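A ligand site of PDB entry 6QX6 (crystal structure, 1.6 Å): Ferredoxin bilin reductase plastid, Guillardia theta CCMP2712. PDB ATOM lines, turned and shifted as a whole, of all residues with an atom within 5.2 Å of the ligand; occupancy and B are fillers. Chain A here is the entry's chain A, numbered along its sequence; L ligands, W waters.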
ATOM      1  N   ALA A  72      -5.546 -32.582 -29.396  1.00  0.00           N
ATOM      2  CA  ALA A  72      -6.520 -32.617 -30.484  1.00  0.00           C
ATOM      3  C   ALA A  72      -6.436 -31.264 -31.185  1.00  0.00           C
ATOM      4  O   ALA A  72      -6.619 -30.224 -30.548  1.00  0.00           O
ATOM      5  CB  ALA A  72      -7.931 -32.887 -29.966  1.00  0.00           C
ATOM      6  N   VAL A  74      -8.140 -29.285 -34.105  1.00  0.00           N
ATOM      7  CA  VAL A  74      -9.340 -29.270 -34.931  1.00  0.00           C
ATOM      8  C   VAL A  74      -9.275 -28.085 -35.875  1.00  0.00           C
ATOM      9  O   VAL A  74      -9.008 -26.948 -35.439  1.00  0.00           O
ATOM     10  CB  VAL A  74     -10.611 -29.214 -34.071  1.00  0.00           C
ATOM     11  CG1 VAL A  74     -11.856 -29.431 -34.937  1.00  0.00           C
ATOM     12  CG2 VAL A  74     -10.538 -30.222 -32.939  1.00  0.00           C
ATOM     13  N   VAL A  82      -9.476 -25.412 -33.045  1.00  0.00           N
ATOM     14  CA  VAL A  82      -9.231 -25.762 -31.657  1.00  0.00           C
ATOM     15  C   VAL A  82      -7.861 -26.412 -31.553  1.00  0.00           C
ATOM     16  O   VAL A  82      -7.492 -27.248 -32.391  1.00  0.00           O
ATOM     17  CB  VAL A  82     -10.314 -26.702 -31.089  1.00  0.00           C
ATOM     18  CG1 VAL A  82      -9.961 -27.138 -29.678  1.00  0.00           C
ATOM     19  CG2 VAL A  82     -11.690 -26.020 -31.121  1.00  0.00           C
ATOM     20  N   ASN A  84      -6.407 -28.383 -28.328  1.00  0.00           N
ATOM     21  CA  ASN A  84      -6.635 -28.881 -26.981  1.00  0.00           C
ATOM     22  C   ASN A  84      -5.413 -29.714 -26.620  1.00  0.00           C
ATOM     23  O   ASN A  84      -5.277 -30.852 -27.064  1.00  0.00           O
ATOM     24  CB  ASN A  84      -7.923 -29.701 -26.911  1.00  0.00           C
ATOM     25  CG  ASN A  84      -8.263 -30.158 -25.506  1.00  0.00           C
ATOM     26  OD1 ASN A  84      -7.410 -30.663 -24.780  1.00  0.00           O
ATOM     27  ND2 ASN A  84      -9.519 -29.992 -25.125  1.00  0.00           N
ATOM     28  N   ASP A 101      -6.251 -24.904 -23.642  1.00  0.00           N
ATOM     29  CA  ASP A 101      -7.457 -24.953 -24.475  1.00  0.00           C
ATOM     30  C   ASP A 101      -7.509 -23.671 -25.272  1.00  0.00           C
ATOM     31  O   ASP A 101      -7.695 -22.585 -24.696  1.00  0.00           O
ATOM     32  CB  ASP A 101      -8.717 -25.119 -23.635  1.00  0.00           C
ATOM     33  CG  ASP A 101      -8.951 -26.548 -23.197  1.00  0.00           C
ATOM     34  OD1 ASP A 101      -8.282 -27.006 -22.252  1.00  0.00           O
ATOM     35  OD2 ASP A 101      -9.823 -27.209 -23.818  1.00  0.00           O
ATOM     36  N   VAL A 103      -9.588 -22.046 -28.388  1.00  0.00           N
ATOM     37  CA  VAL A 103     -10.795 -22.276 -29.177  1.00  0.00           C
ATOM     38  C   VAL A 103     -11.122 -21.023 -29.960  1.00  0.00           C
ATOM     39  O   VAL A 103     -11.175 -19.922 -29.406  1.00  0.00           O
ATOM     40  CB  VAL A 103     -11.976 -22.679 -28.270  1.00  0.00           C
ATOM     41  CG1 VAL A 103     -13.242 -22.829 -29.086  1.00  0.00           C
ATOM     42  CG2 VAL A 103     -11.649 -23.968 -27.518  1.00  0.00           C
ATOM     43  N   LEU A 105     -14.122 -19.695 -32.515  1.00  0.00           N
ATOM     44  CA  LEU A 105     -15.465 -19.942 -33.011  1.00  0.00           C
ATOM     45  C   LEU A 105     -15.940 -18.704 -33.771  1.00  0.00           C
ATOM     46  O   LEU A 105     -15.248 -17.677 -33.768  1.00  0.00           O
ATOM     47  CB  LEU A 105     -16.405 -20.271 -31.856  1.00  0.00           C
ATOM     48  CG  LEU A 105     -16.101 -21.587 -31.141  1.00  0.00           C
ATOM     49  CD1 LEU A 105     -16.771 -21.631 -29.785  1.00  0.00           C
ATOM     50  CD2 LEU A 105     -16.553 -22.769 -32.007  1.00  0.00           C
ATOM     51  N   LEU A 110     -11.674 -18.155 -27.507  1.00  0.00           N
ATOM     52  CA  LEU A 110     -11.711 -18.557 -26.100  1.00  0.00           C
ATOM     53  C   LEU A 110     -10.374 -19.187 -25.751  1.00  0.00           C
ATOM     54  O   LEU A 110      -9.926 -20.110 -26.429  1.00  0.00           O
ATOM     55  CB  LEU A 110     -12.839 -19.569 -25.831  1.00  0.00           C
ATOM     56  CG  LEU A 110     -14.304 -19.137 -25.949  1.00  0.00           C
ATOM     57  CD1 LEU A 110     -14.835 -19.297 -27.360  1.00  0.00           C
ATOM     58  CD2 LEU A 110     -15.133 -19.953 -24.964  1.00  0.00           C
ATOM     59  N   ALA A 112      -7.990 -20.730 -22.574  1.00  0.00           N
ATOM     60  CA  ALA A 112      -7.857 -21.208 -21.206  1.00  0.00           C
ATOM     61  C   ALA A 112      -6.491 -21.878 -21.056  1.00  0.00           C
ATOM     62  O   ALA A 112      -6.261 -22.955 -21.611  1.00  0.00           O
ATOM     63  CB  ALA A 112      -8.974 -22.193 -20.847  1.00  0.00           C
ATOM     64  N   GLN A 116      -3.466 -26.694 -13.928  1.00  0.00           N
ATOM     65  CA  GLN A 116      -4.624 -27.054 -13.125  1.00  0.00           C
ATOM     66  C   GLN A 116      -4.178 -27.891 -11.932  1.00  0.00           C
ATOM     67  O   GLN A 116      -3.553 -28.945 -12.125  1.00  0.00           O
ATOM     68  CB  GLN A 116      -5.625 -27.770 -14.005  1.00  0.00           C
ATOM     69  CG  GLN A 116      -6.037 -26.907 -15.213  1.00  0.00           C
ATOM     70  CD  GLN A 116      -6.866 -27.633 -16.237  1.00  0.00           C
ATOM     71  OE1 GLN A 116      -6.336 -28.371 -17.076  1.00  0.00           O
ATOM     72  NE2 GLN A 116      -8.178 -27.432 -16.197  1.00  0.00           N
ATOM     73  N   ASP A 148     -17.492 -14.723 -17.215  1.00  0.00           N
ATOM     74  CA  ASP A 148     -18.278 -15.729 -16.523  1.00  0.00           C
ATOM     75  C   ASP A 148     -17.726 -17.125 -16.785  1.00  0.00           C
ATOM     76  O   ASP A 148     -17.258 -17.441 -17.879  1.00  0.00           O
ATOM     77  CB  ASP A 148     -19.741 -15.643 -16.954  1.00  0.00           C
ATOM     78  CG  ASP A 148     -20.501 -14.567 -16.209  1.00  0.00           C
ATOM     79  OD1 ASP A 148     -20.295 -14.438 -14.989  1.00  0.00           O
ATOM     80  OD2 ASP A 148     -21.278 -13.840 -16.858  1.00  0.00           O
ATOM     81  N   PHE A 149     -17.795 -17.980 -15.761  1.00  0.00           N
ATOM     82  CA  PHE A 149     -17.108 -19.256 -15.758  1.00  0.00           C
ATOM     83  C   PHE A 149     -17.912 -20.305 -14.994  1.00  0.00           C
ATOM     84  O   PHE A 149     -18.394 -20.019 -13.897  1.00  0.00           O
ATOM     85  CB  PHE A 149     -15.736 -19.061 -15.101  1.00  0.00           C
ATOM     86  CG  PHE A 149     -14.730 -20.090 -15.500  1.00  0.00           C
ATOM     87  CD1 PHE A 149     -14.176 -20.079 -16.767  1.00  0.00           C
ATOM     88  CD2 PHE A 149     -14.327 -21.073 -14.605  1.00  0.00           C
ATOM     89  CE1 PHE A 149     -13.256 -21.015 -17.138  1.00  0.00           C
ATOM     90  CE2 PHE A 149     -13.407 -22.022 -14.979  1.00  0.00           C
ATOM     91  CZ  PHE A 149     -12.868 -21.995 -16.251  1.00  0.00           C
ATOM     92  N   PRO A 150     -18.054 -21.514 -15.538  1.00  0.00           N
ATOM     93  CA  PRO A 150     -18.883 -22.519 -14.854  1.00  0.00           C
ATOM     94  C   PRO A 150     -18.377 -22.821 -13.444  1.00  0.00           C
ATOM     95  O   PRO A 150     -17.183 -23.006 -13.225  1.00  0.00           O
ATOM     96  CB  PRO A 150     -18.812 -23.755 -15.768  1.00  0.00           C
ATOM     97  CG  PRO A 150     -17.885 -23.426 -16.870  1.00  0.00           C
ATOM     98  CD  PRO A 150     -17.563 -21.976 -16.849  1.00  0.00           C
ATOM     99  N   ALA A 153     -16.295 -26.041 -12.313  1.00  0.00           N
ATOM    100  CA  ALA A 153     -14.939 -26.106 -12.816  1.00  0.00           C
ATOM    101  C   ALA A 153     -13.947 -25.331 -11.962  1.00  0.00           C
ATOM    102  O   ALA A 153     -12.737 -25.537 -12.092  1.00  0.00           O
ATOM    103  CB  ALA A 153     -14.892 -25.578 -14.251  1.00  0.00           C
ATOM    104  N   TYR A 156     -10.812 -26.722 -10.157  1.00  0.00           N
ATOM    105  CA  TYR A 156      -9.760 -27.315 -10.968  1.00  0.00           C
ATOM    106  C   TYR A 156      -8.800 -26.289 -11.559  1.00  0.00           C
ATOM    107  O   TYR A 156      -8.020 -26.621 -12.452  1.00  0.00           O
ATOM    108  CB  TYR A 156     -10.358 -28.146 -12.104  1.00  0.00           C
ATOM    109  CG  TYR A 156     -11.299 -29.233 -11.635  1.00  0.00           C
ATOM    110  CD1 TYR A 156     -10.835 -30.268 -10.839  1.00  0.00           C
ATOM    111  CD2 TYR A 156     -12.629 -29.236 -12.003  1.00  0.00           C
ATOM    112  CE1 TYR A 156     -11.681 -31.268 -10.413  1.00  0.00           C
ATOM    113  CE2 TYR A 156     -13.490 -30.220 -11.582  1.00  0.00           C
ATOM    114  CZ  TYR A 156     -13.012 -31.241 -10.783  1.00  0.00           C
ATOM    115  OH  TYR A 156     -13.866 -32.235 -10.354  1.00  0.00           O
ATOM    116  N   PHE A 157      -8.840 -25.038 -11.099  1.00  0.00           N
ATOM    117  CA  PHE A 157      -8.014 -23.995 -11.679  1.00  0.00           C
ATOM    118  C   PHE A 157      -7.196 -23.318 -10.584  1.00  0.00           C
ATOM    119  O   PHE A 157      -7.629 -23.208  -9.434  1.00  0.00           O
ATOM    120  CB  PHE A 157      -8.866 -22.981 -12.442  1.00  0.00           C
ATOM    121  CG  PHE A 157      -9.370 -23.508 -13.748  1.00  0.00           C
ATOM    122  CD1 PHE A 157      -8.548 -23.543 -14.863  1.00  0.00           C
ATOM    123  CD2 PHE A 157     -10.666 -24.004 -13.869  1.00  0.00           C
ATOM    124  CE1 PHE A 157      -9.007 -24.038 -16.069  1.00  0.00           C
ATOM    125  CE2 PHE A 157     -11.125 -24.499 -15.075  1.00  0.00           C
ATOM    126  CZ  PHE A 157     -10.289 -24.522 -16.177  1.00  0.00           C
ATOM    127  N   TRP A 163      -7.547 -16.907 -18.325  1.00  0.00           N
ATOM    128  CA  TRP A 163      -8.862 -17.098 -18.943  1.00  0.00           C
ATOM    129  C   TRP A 163      -9.193 -15.788 -19.637  1.00  0.00           C
ATOM    130  O   TRP A 163      -9.404 -14.771 -18.975  1.00  0.00           O
ATOM    131  CB  TRP A 163      -9.889 -17.490 -17.884  1.00  0.00           C
ATOM    132  CG  TRP A 163     -11.322 -17.318 -18.251  1.00  0.00           C
ATOM    133  CD1 TRP A 163     -12.242 -16.547 -17.604  1.00  0.00           C
ATOM    134  CD2 TRP A 163     -12.014 -17.937 -19.336  1.00  0.00           C
ATOM    135  NE1 TRP A 163     -13.466 -16.644 -18.211  1.00  0.00           N
ATOM    136  CE2 TRP A 163     -13.360 -17.490 -19.289  1.00  0.00           C
ATOM    137  CE3 TRP A 163     -11.643 -18.822 -20.343  1.00  0.00           C
ATOM    138  CZ2 TRP A 163     -14.313 -17.900 -20.211  1.00  0.00           C
ATOM    139  CZ3 TRP A 163     -12.596 -19.232 -21.265  1.00  0.00           C
ATOM    140  CH2 TRP A 163     -13.920 -18.772 -21.184  1.00  0.00           C
ATOM    141  N   ARG A 165     -10.626 -13.764 -23.564  1.00  0.00           N
ATOM    142  CA  ARG A 165     -11.352 -13.819 -24.835  1.00  0.00           C
ATOM    143  C   ARG A 165     -10.789 -12.772 -25.786  1.00  0.00           C
ATOM    144  O   ARG A 165     -11.371 -11.681 -25.938  1.00  0.00           O
ATOM    145  CB  ARG A 165     -12.850 -13.587 -24.622  1.00  0.00           C
ATOM    146  CG  ARG A 165     -13.515 -14.617 -23.734  1.00  0.00           C
ATOM    147  CD  ARG A 165     -14.957 -14.232 -23.440  1.00  0.00           C
ATOM    148  NE  ARG A 165     -15.662 -15.262 -22.686  1.00  0.00           N
ATOM    149  CZ  ARG A 165     -16.203 -16.344 -23.229  1.00  0.00           C
ATOM    150  NH1 ARG A 165     -16.107 -16.552 -24.546  1.00  0.00           N
ATOM    151  NH2 ARG A 165     -16.834 -17.235 -22.471  1.00  0.00           N
ATOM    152  N   TYR A 213     -10.713 -34.763 -11.582  1.00  0.00           N
ATOM    153  CA  TYR A 213     -10.514 -33.869 -12.715  1.00  0.00           C
ATOM    154  C   TYR A 213     -10.845 -34.553 -14.030  1.00  0.00           C
ATOM    155  O   TYR A 213     -11.575 -34.015 -14.868  1.00  0.00           O
ATOM    156  CB  TYR A 213      -9.067 -33.352 -12.720  1.00  0.00           C
ATOM    157  CG  TYR A 213      -8.714 -32.498 -13.912  1.00  0.00           C
ATOM    158  CD1 TYR A 213      -9.208 -31.213 -14.046  1.00  0.00           C
ATOM    159  CD2 TYR A 213      -7.869 -32.988 -14.894  1.00  0.00           C
ATOM    160  CE1 TYR A 213      -8.878 -30.430 -15.143  1.00  0.00           C
ATOM    161  CE2 TYR A 213      -7.532 -32.212 -15.993  1.00  0.00           C
ATOM    162  CZ  TYR A 213      -8.046 -30.939 -16.108  1.00  0.00           C
ATOM    163  OH  TYR A 213      -7.701 -30.172 -17.200  1.00  0.00           O
ATOM    164  N   TYR A 216     -14.603 -35.031 -14.485  1.00  0.00           N
ATOM    165  CA  TYR A 216     -15.329 -33.804 -14.790  1.00  0.00           C
ATOM    166  C   TYR A 216     -15.215 -33.448 -16.265  1.00  0.00           C
ATOM    167  O   TYR A 216     -16.224 -33.159 -16.930  1.00  0.00           O
ATOM    168  CB  TYR A 216     -14.813 -32.640 -13.932  1.00  0.00           C
ATOM    169  CG  TYR A 216     -15.465 -31.329 -14.301  1.00  0.00           C
ATOM    170  CD1 TYR A 216     -16.691 -30.957 -13.761  1.00  0.00           C
ATOM    171  CD2 TYR A 216     -14.875 -30.463 -15.210  1.00  0.00           C
ATOM    172  CE1 TYR A 216     -17.290 -29.763 -14.102  1.00  0.00           C
ATOM    173  CE2 TYR A 216     -15.460 -29.265 -15.561  1.00  0.00           C
ATOM    174  CZ  TYR A 216     -16.678 -28.919 -15.008  1.00  0.00           C
ATOM    175  OH  TYR A 216     -17.270 -27.732 -15.351  1.00  0.00           O
ATOM    176  N   ARG A 217     -13.990 -33.445 -16.806  1.00  0.00           N
ATOM    177  CA  ARG A 217     -13.804 -33.013 -18.180  1.00  0.00           C
ATOM    178  C   ARG A 217     -14.384 -34.027 -19.159  1.00  0.00           C
ATOM    179  O   ARG A 217     -14.914 -33.640 -20.213  1.00  0.00           O
ATOM    180  CB  ARG A 217     -12.327 -32.776 -18.470  1.00  0.00           C
ATOM    181  CG  ARG A 217     -11.786 -31.500 -17.832  1.00  0.00           C
ATOM    182  CD  ARG A 217     -10.521 -31.016 -18.522  1.00  0.00           C
ATOM    183  NE  ARG A 217     -10.796 -30.399 -19.815  1.00  0.00           N
ATOM    184  CZ  ARG A 217      -9.868 -29.933 -20.641  1.00  0.00           C
ATOM    185  NH1 ARG A 217      -8.587 -30.004 -20.301  1.00  0.00           N
ATOM    186  NH2 ARG A 217     -10.207 -29.385 -21.794  1.00  0.00           N
ATOM    187  N   ASP A 221     -16.817 -31.366 -20.511  1.00  0.00           N
ATOM    188  CA  ASP A 221     -16.049 -30.486 -21.383  1.00  0.00           C
ATOM    189  C   ASP A 221     -16.910 -30.081 -22.572  1.00  0.00           C
ATOM    190  O   ASP A 221     -17.565 -30.933 -23.183  1.00  0.00           O
ATOM    191  CB  ASP A 221     -14.769 -31.186 -21.849  1.00  0.00           C
ATOM    192  CG  ASP A 221     -13.781 -30.201 -22.452  1.00  0.00           C
ATOM    193  OD1 ASP A 221     -14.110 -29.577 -23.481  1.00  0.00           O
ATOM    194  OD2 ASP A 221     -12.680 -30.045 -21.877  1.00  0.00           O
ATOM    195  N   PRO A 222     -16.938 -28.793 -22.934  1.00  0.00           N
ATOM    196  CA  PRO A 222     -17.748 -28.375 -24.091  1.00  0.00           C
ATOM    197  C   PRO A 222     -17.323 -29.031 -25.390  1.00  0.00           C
ATOM    198  O   PRO A 222     -18.076 -28.983 -26.371  1.00  0.00           O
ATOM    199  CB  PRO A 222     -17.550 -26.858 -24.129  1.00  0.00           C
ATOM    200  CG  PRO A 222     -17.194 -26.492 -22.726  1.00  0.00           C
ATOM    201  CD  PRO A 222     -16.357 -27.629 -22.234  1.00  0.00           C
ATOM    202  N   ALA A 223     -16.129 -29.640 -25.444  1.00  0.00           N
ATOM    203  CA  ALA A 223     -15.719 -30.363 -26.636  1.00  0.00           C
ATOM    204  C   ALA A 223     -16.727 -31.450 -26.995  1.00  0.00           C
ATOM    205  O   ALA A 223     -16.921 -31.743 -28.177  1.00  0.00           O
ATOM    206  CB  ALA A 223     -14.331 -30.982 -26.432  1.00  0.00           C
ATOM    207  N   MET A 226     -19.422 -30.092 -29.326  1.00  0.00           N
ATOM    208  CA  MET A 226     -18.943 -29.720 -30.657  1.00  0.00           C
ATOM    209  C   MET A 226     -18.571 -30.952 -31.468  1.00  0.00           C
ATOM    210  O   MET A 226     -18.918 -31.048 -32.653  1.00  0.00           O
ATOM    211  CB  MET A 226     -17.742 -28.774 -30.522  1.00  0.00           C
ATOM    212  CG  MET A 226     -17.388 -28.071 -31.808  1.00  0.00           C
ATOM    213  SD  MET A 226     -18.800 -27.165 -32.473  1.00  0.00           S
ATOM    214  CE  MET A 226     -18.929 -25.796 -31.323  1.00  0.00           C
ATOM    215  N   PHE A 227     -17.861 -31.903 -30.858  1.00  0.00           N
ATOM    216  CA  PHE A 227     -17.506 -33.128 -31.563  1.00  0.00           C
ATOM    217  C   PHE A 227     -18.757 -33.901 -31.980  1.00  0.00           C
ATOM    218  O   PHE A 227     -18.770 -34.516 -33.052  1.00  0.00           O
ATOM    219  CB  PHE A 227     -16.611 -34.012 -30.683  1.00  0.00           C
ATOM    220  CG  PHE A 227     -15.155 -33.613 -30.710  1.00  0.00           C
ATOM    221  CD1 PHE A 227     -14.505 -33.371 -31.907  1.00  0.00           C
ATOM    222  CD2 PHE A 227     -14.448 -33.491 -29.524  1.00  0.00           C
ATOM    223  CE1 PHE A 227     -13.176 -33.018 -31.931  1.00  0.00           C
ATOM    224  CE2 PHE A 227     -13.112 -33.131 -29.546  1.00  0.00           C
ATOM    225  CZ  PHE A 227     -12.469 -32.896 -30.745  1.00  0.00           C
ATOM    226  N   MET A 230     -20.117 -32.457 -35.074  1.00  0.00           N
ATOM    227  CA  MET A 230     -19.199 -32.660 -36.187  1.00  0.00           C
ATOM    228  C   MET A 230     -19.212 -34.112 -36.668  1.00  0.00           C
ATOM    229  O   MET A 230     -19.295 -34.367 -37.877  1.00  0.00           O
ATOM    230  CB  MET A 230     -17.798 -32.248 -35.782  1.00  0.00           C
ATOM    231  CG  MET A 230     -17.560 -30.758 -35.695  1.00  0.00           C
ATOM    232  SD  MET A 230     -15.949 -30.394 -35.001  1.00  0.00           S
ATOM    233  CE  MET A 230     -14.889 -30.761 -36.394  1.00  0.00           C
HETATM  234  N1  LIG L   1     -13.130 -27.138 -26.621  1.00  0.00           N
HETATM  235  C1  LIG L   1     -12.169 -28.114 -26.870  1.00  0.00           C
HETATM  236  C2  LIG L   1     -12.523 -28.717 -28.183  1.00  0.00           C
HETATM  237  C3  LIG L   1     -13.631 -28.101 -28.660  1.00  0.00           C
HETATM  238  C4  LIG L   1     -14.056 -27.094 -27.700  1.00  0.00           C
HETATM  239  C5  LIG L   1     -11.677 -29.784 -28.721  1.00  0.00           C
HETATM  240  C6  LIG L   1     -14.143 -29.451 -30.649  1.00  0.00           C
HETATM  241  O1  LIG L   1     -11.242 -28.395 -26.126  1.00  0.00           O
HETATM  242  C7  LIG L   1     -15.106 -26.298 -27.840  1.00  0.00           C
HETATM  243  C8  LIG L   1     -14.345 -28.355 -29.923  1.00  0.00           C
HETATM  244  N2  LIG L   1     -15.073 -25.004 -25.638  1.00  0.00           N
HETATM  245  C9  LIG L   1     -15.607 -25.370 -26.888  1.00  0.00           C
HETATM  246  C10 LIG L   1     -16.764 -24.636 -27.103  1.00  0.00           C
HETATM  247  C11 LIG L   1     -16.982 -23.825 -26.009  1.00  0.00           C
HETATM  248  C12 LIG L   1     -15.945 -24.042 -25.097  1.00  0.00           C
HETATM  249  C13 LIG L   1     -15.820 -23.384 -23.831  1.00  0.00           C
HETATM  250  C14 LIG L   1     -17.621 -24.725 -28.283  1.00  0.00           C
HETATM  251  C15 LIG L   1     -18.085 -22.896 -25.809  1.00  0.00           C
HETATM  252  C16 LIG L   1     -19.271 -23.614 -25.196  1.00  0.00           C
HETATM  253  C17 LIG L   1     -20.378 -22.610 -24.871  1.00  0.00           C
HETATM  254  O2  LIG L   1     -20.273 -21.444 -25.345  1.00  0.00           O
HETATM  255  O3  LIG L   1     -21.319 -23.010 -24.151  1.00  0.00           O
HETATM  256  C18 LIG L   1     -11.954 -24.855 -21.115  1.00  0.00           C
HETATM  257  N3  LIG L   1     -13.708 -24.388 -22.861  1.00  0.00           N
HETATM  258  C19 LIG L   1     -14.921 -23.595 -22.839  1.00  0.00           C
HETATM  259  C20 LIG L   1     -15.048 -22.980 -21.533  1.00  0.00           C
HETATM  260  C21 LIG L   1     -13.999 -23.386 -20.787  1.00  0.00           C
HETATM  261  C22 LIG L   1     -13.197 -24.240 -21.618  1.00  0.00           C
HETATM  262  C23 LIG L   1     -13.722 -23.020 -19.412  1.00  0.00           C
HETATM  263  C24 LIG L   1     -16.171 -22.132 -21.147  1.00  0.00           C
HETATM  264  C25 LIG L   1     -17.376 -23.070 -20.988  1.00  0.00           C
HETATM  265  C26 LIG L   1     -18.632 -22.352 -20.456  1.00  0.00           C
HETATM  266  O4  LIG L   1     -19.569 -23.075 -20.032  1.00  0.00           O
HETATM  267  O5  LIG L   1     -18.632 -21.100 -20.475  1.00  0.00           O
HETATM  268  N4  LIG L   1     -10.982 -26.923 -20.221  1.00  0.00           N
HETATM  269  C27 LIG L   1     -12.256 -26.268 -20.577  1.00  0.00           C
HETATM  270  C28 LIG L   1     -13.018 -26.314 -19.248  1.00  0.00           C
HETATM  271  C29 LIG L   1     -12.275 -26.944 -18.312  1.00  0.00           C
HETATM  272  C30 LIG L   1     -10.972 -27.324 -18.899  1.00  0.00           C
HETATM  273  C31 LIG L   1     -14.463 -26.057 -19.124  1.00  0.00           C
HETATM  274  C32 LIG L   1     -12.768 -27.521 -17.089  1.00  0.00           C
HETATM  275  C33 LIG L   1     -11.971 -28.044 -16.168  1.00  0.00           C
HETATM  276  O6  LIG L   1     -10.013 -27.885 -18.390  1.00  0.00           O
HETATM  277  O   HOH W   1     -12.818 -26.886 -24.033  1.00  0.00           O
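Water W1 lies within hydrogen-bond range of a nitrogen (N1) of the ligand (2.6 Å), the side-chain carboxylate of Asp 101 (3.0 Å) and the side-chain carboxylate of Asp 221 (3.0 Å).
ND2 of Asn 84 is in hydrogen-bond range of O1 of the ligand, 2.6 Å away.
An oxygen (O6) of the ligand lies within hydrogen-bond range of the side-chain amide nitrogen (NE2) of Gln 116 (2.9 Å).
OD1 of Asp 101 sits at hydrogen-bond distance from N4 of the ligand.
The guanidinium group of Arg 217 sits at hydrogen-bond distance from an oxygen (O6) of the ligand (3.0 Å).
OH of Tyr 213 is in hydrogen-bond range of O6 of the ligand, at 3.5 Å.
Merely in contact with the ligand: Phe 149 (3.1 Å), Val 82 (3.3 Å), Pro 222 (3.4 Å), Ala 223 (3.4 Å), Met 226 (3.5 Å), Leu 105 (3.5 Å), Tyr 216 (3.6 Å), Pro 150 (3.6 Å), Val 103 (3.6 Å), Leu 110 (3.7 Å), Phe 227 (3.7 Å), Phe 157 (3.8 Å) and Asp 221 (3.9 Å).
The nearest printed residue that does not touch the ligand is Ala 112 (4.005 Å).
The side-chain amide nitrogen (ND2) of Asn 84 is in hydrogen-bond range of the side-chain carboxylate (OD2) of Asp 101.
ND2 of Asn 84 lies close to NH2 of Arg 217 (3.5 Å).
NE2 of Gln 116 sits close to OH of Tyr 213 (3.0 Å).
The backbone carbonyl oxygen (O) of Ala 112 lies within hydrogen-bond range of the backbone NH (N) of Asp 101, 2.8 Å away.
The guanidinium group (NH1) of Arg 217 lies close to the side-chain hydroxyl (OH) of Tyr 213, at 3.2 Å.
The backbone NH (N) of Val 74 sits at hydrogen-bond distance from the backbone carbonyl oxygen (O) of Val 82 (2.7 Å).
N of Ala 223 lies within hydrogen-bond range of OD1 of Asp 221 (2.8 Å).
The backbone NH of Leu 110 is in hydrogen-bond range of the backbone carbonyl oxygen of Val 103, 2.6 Å away.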
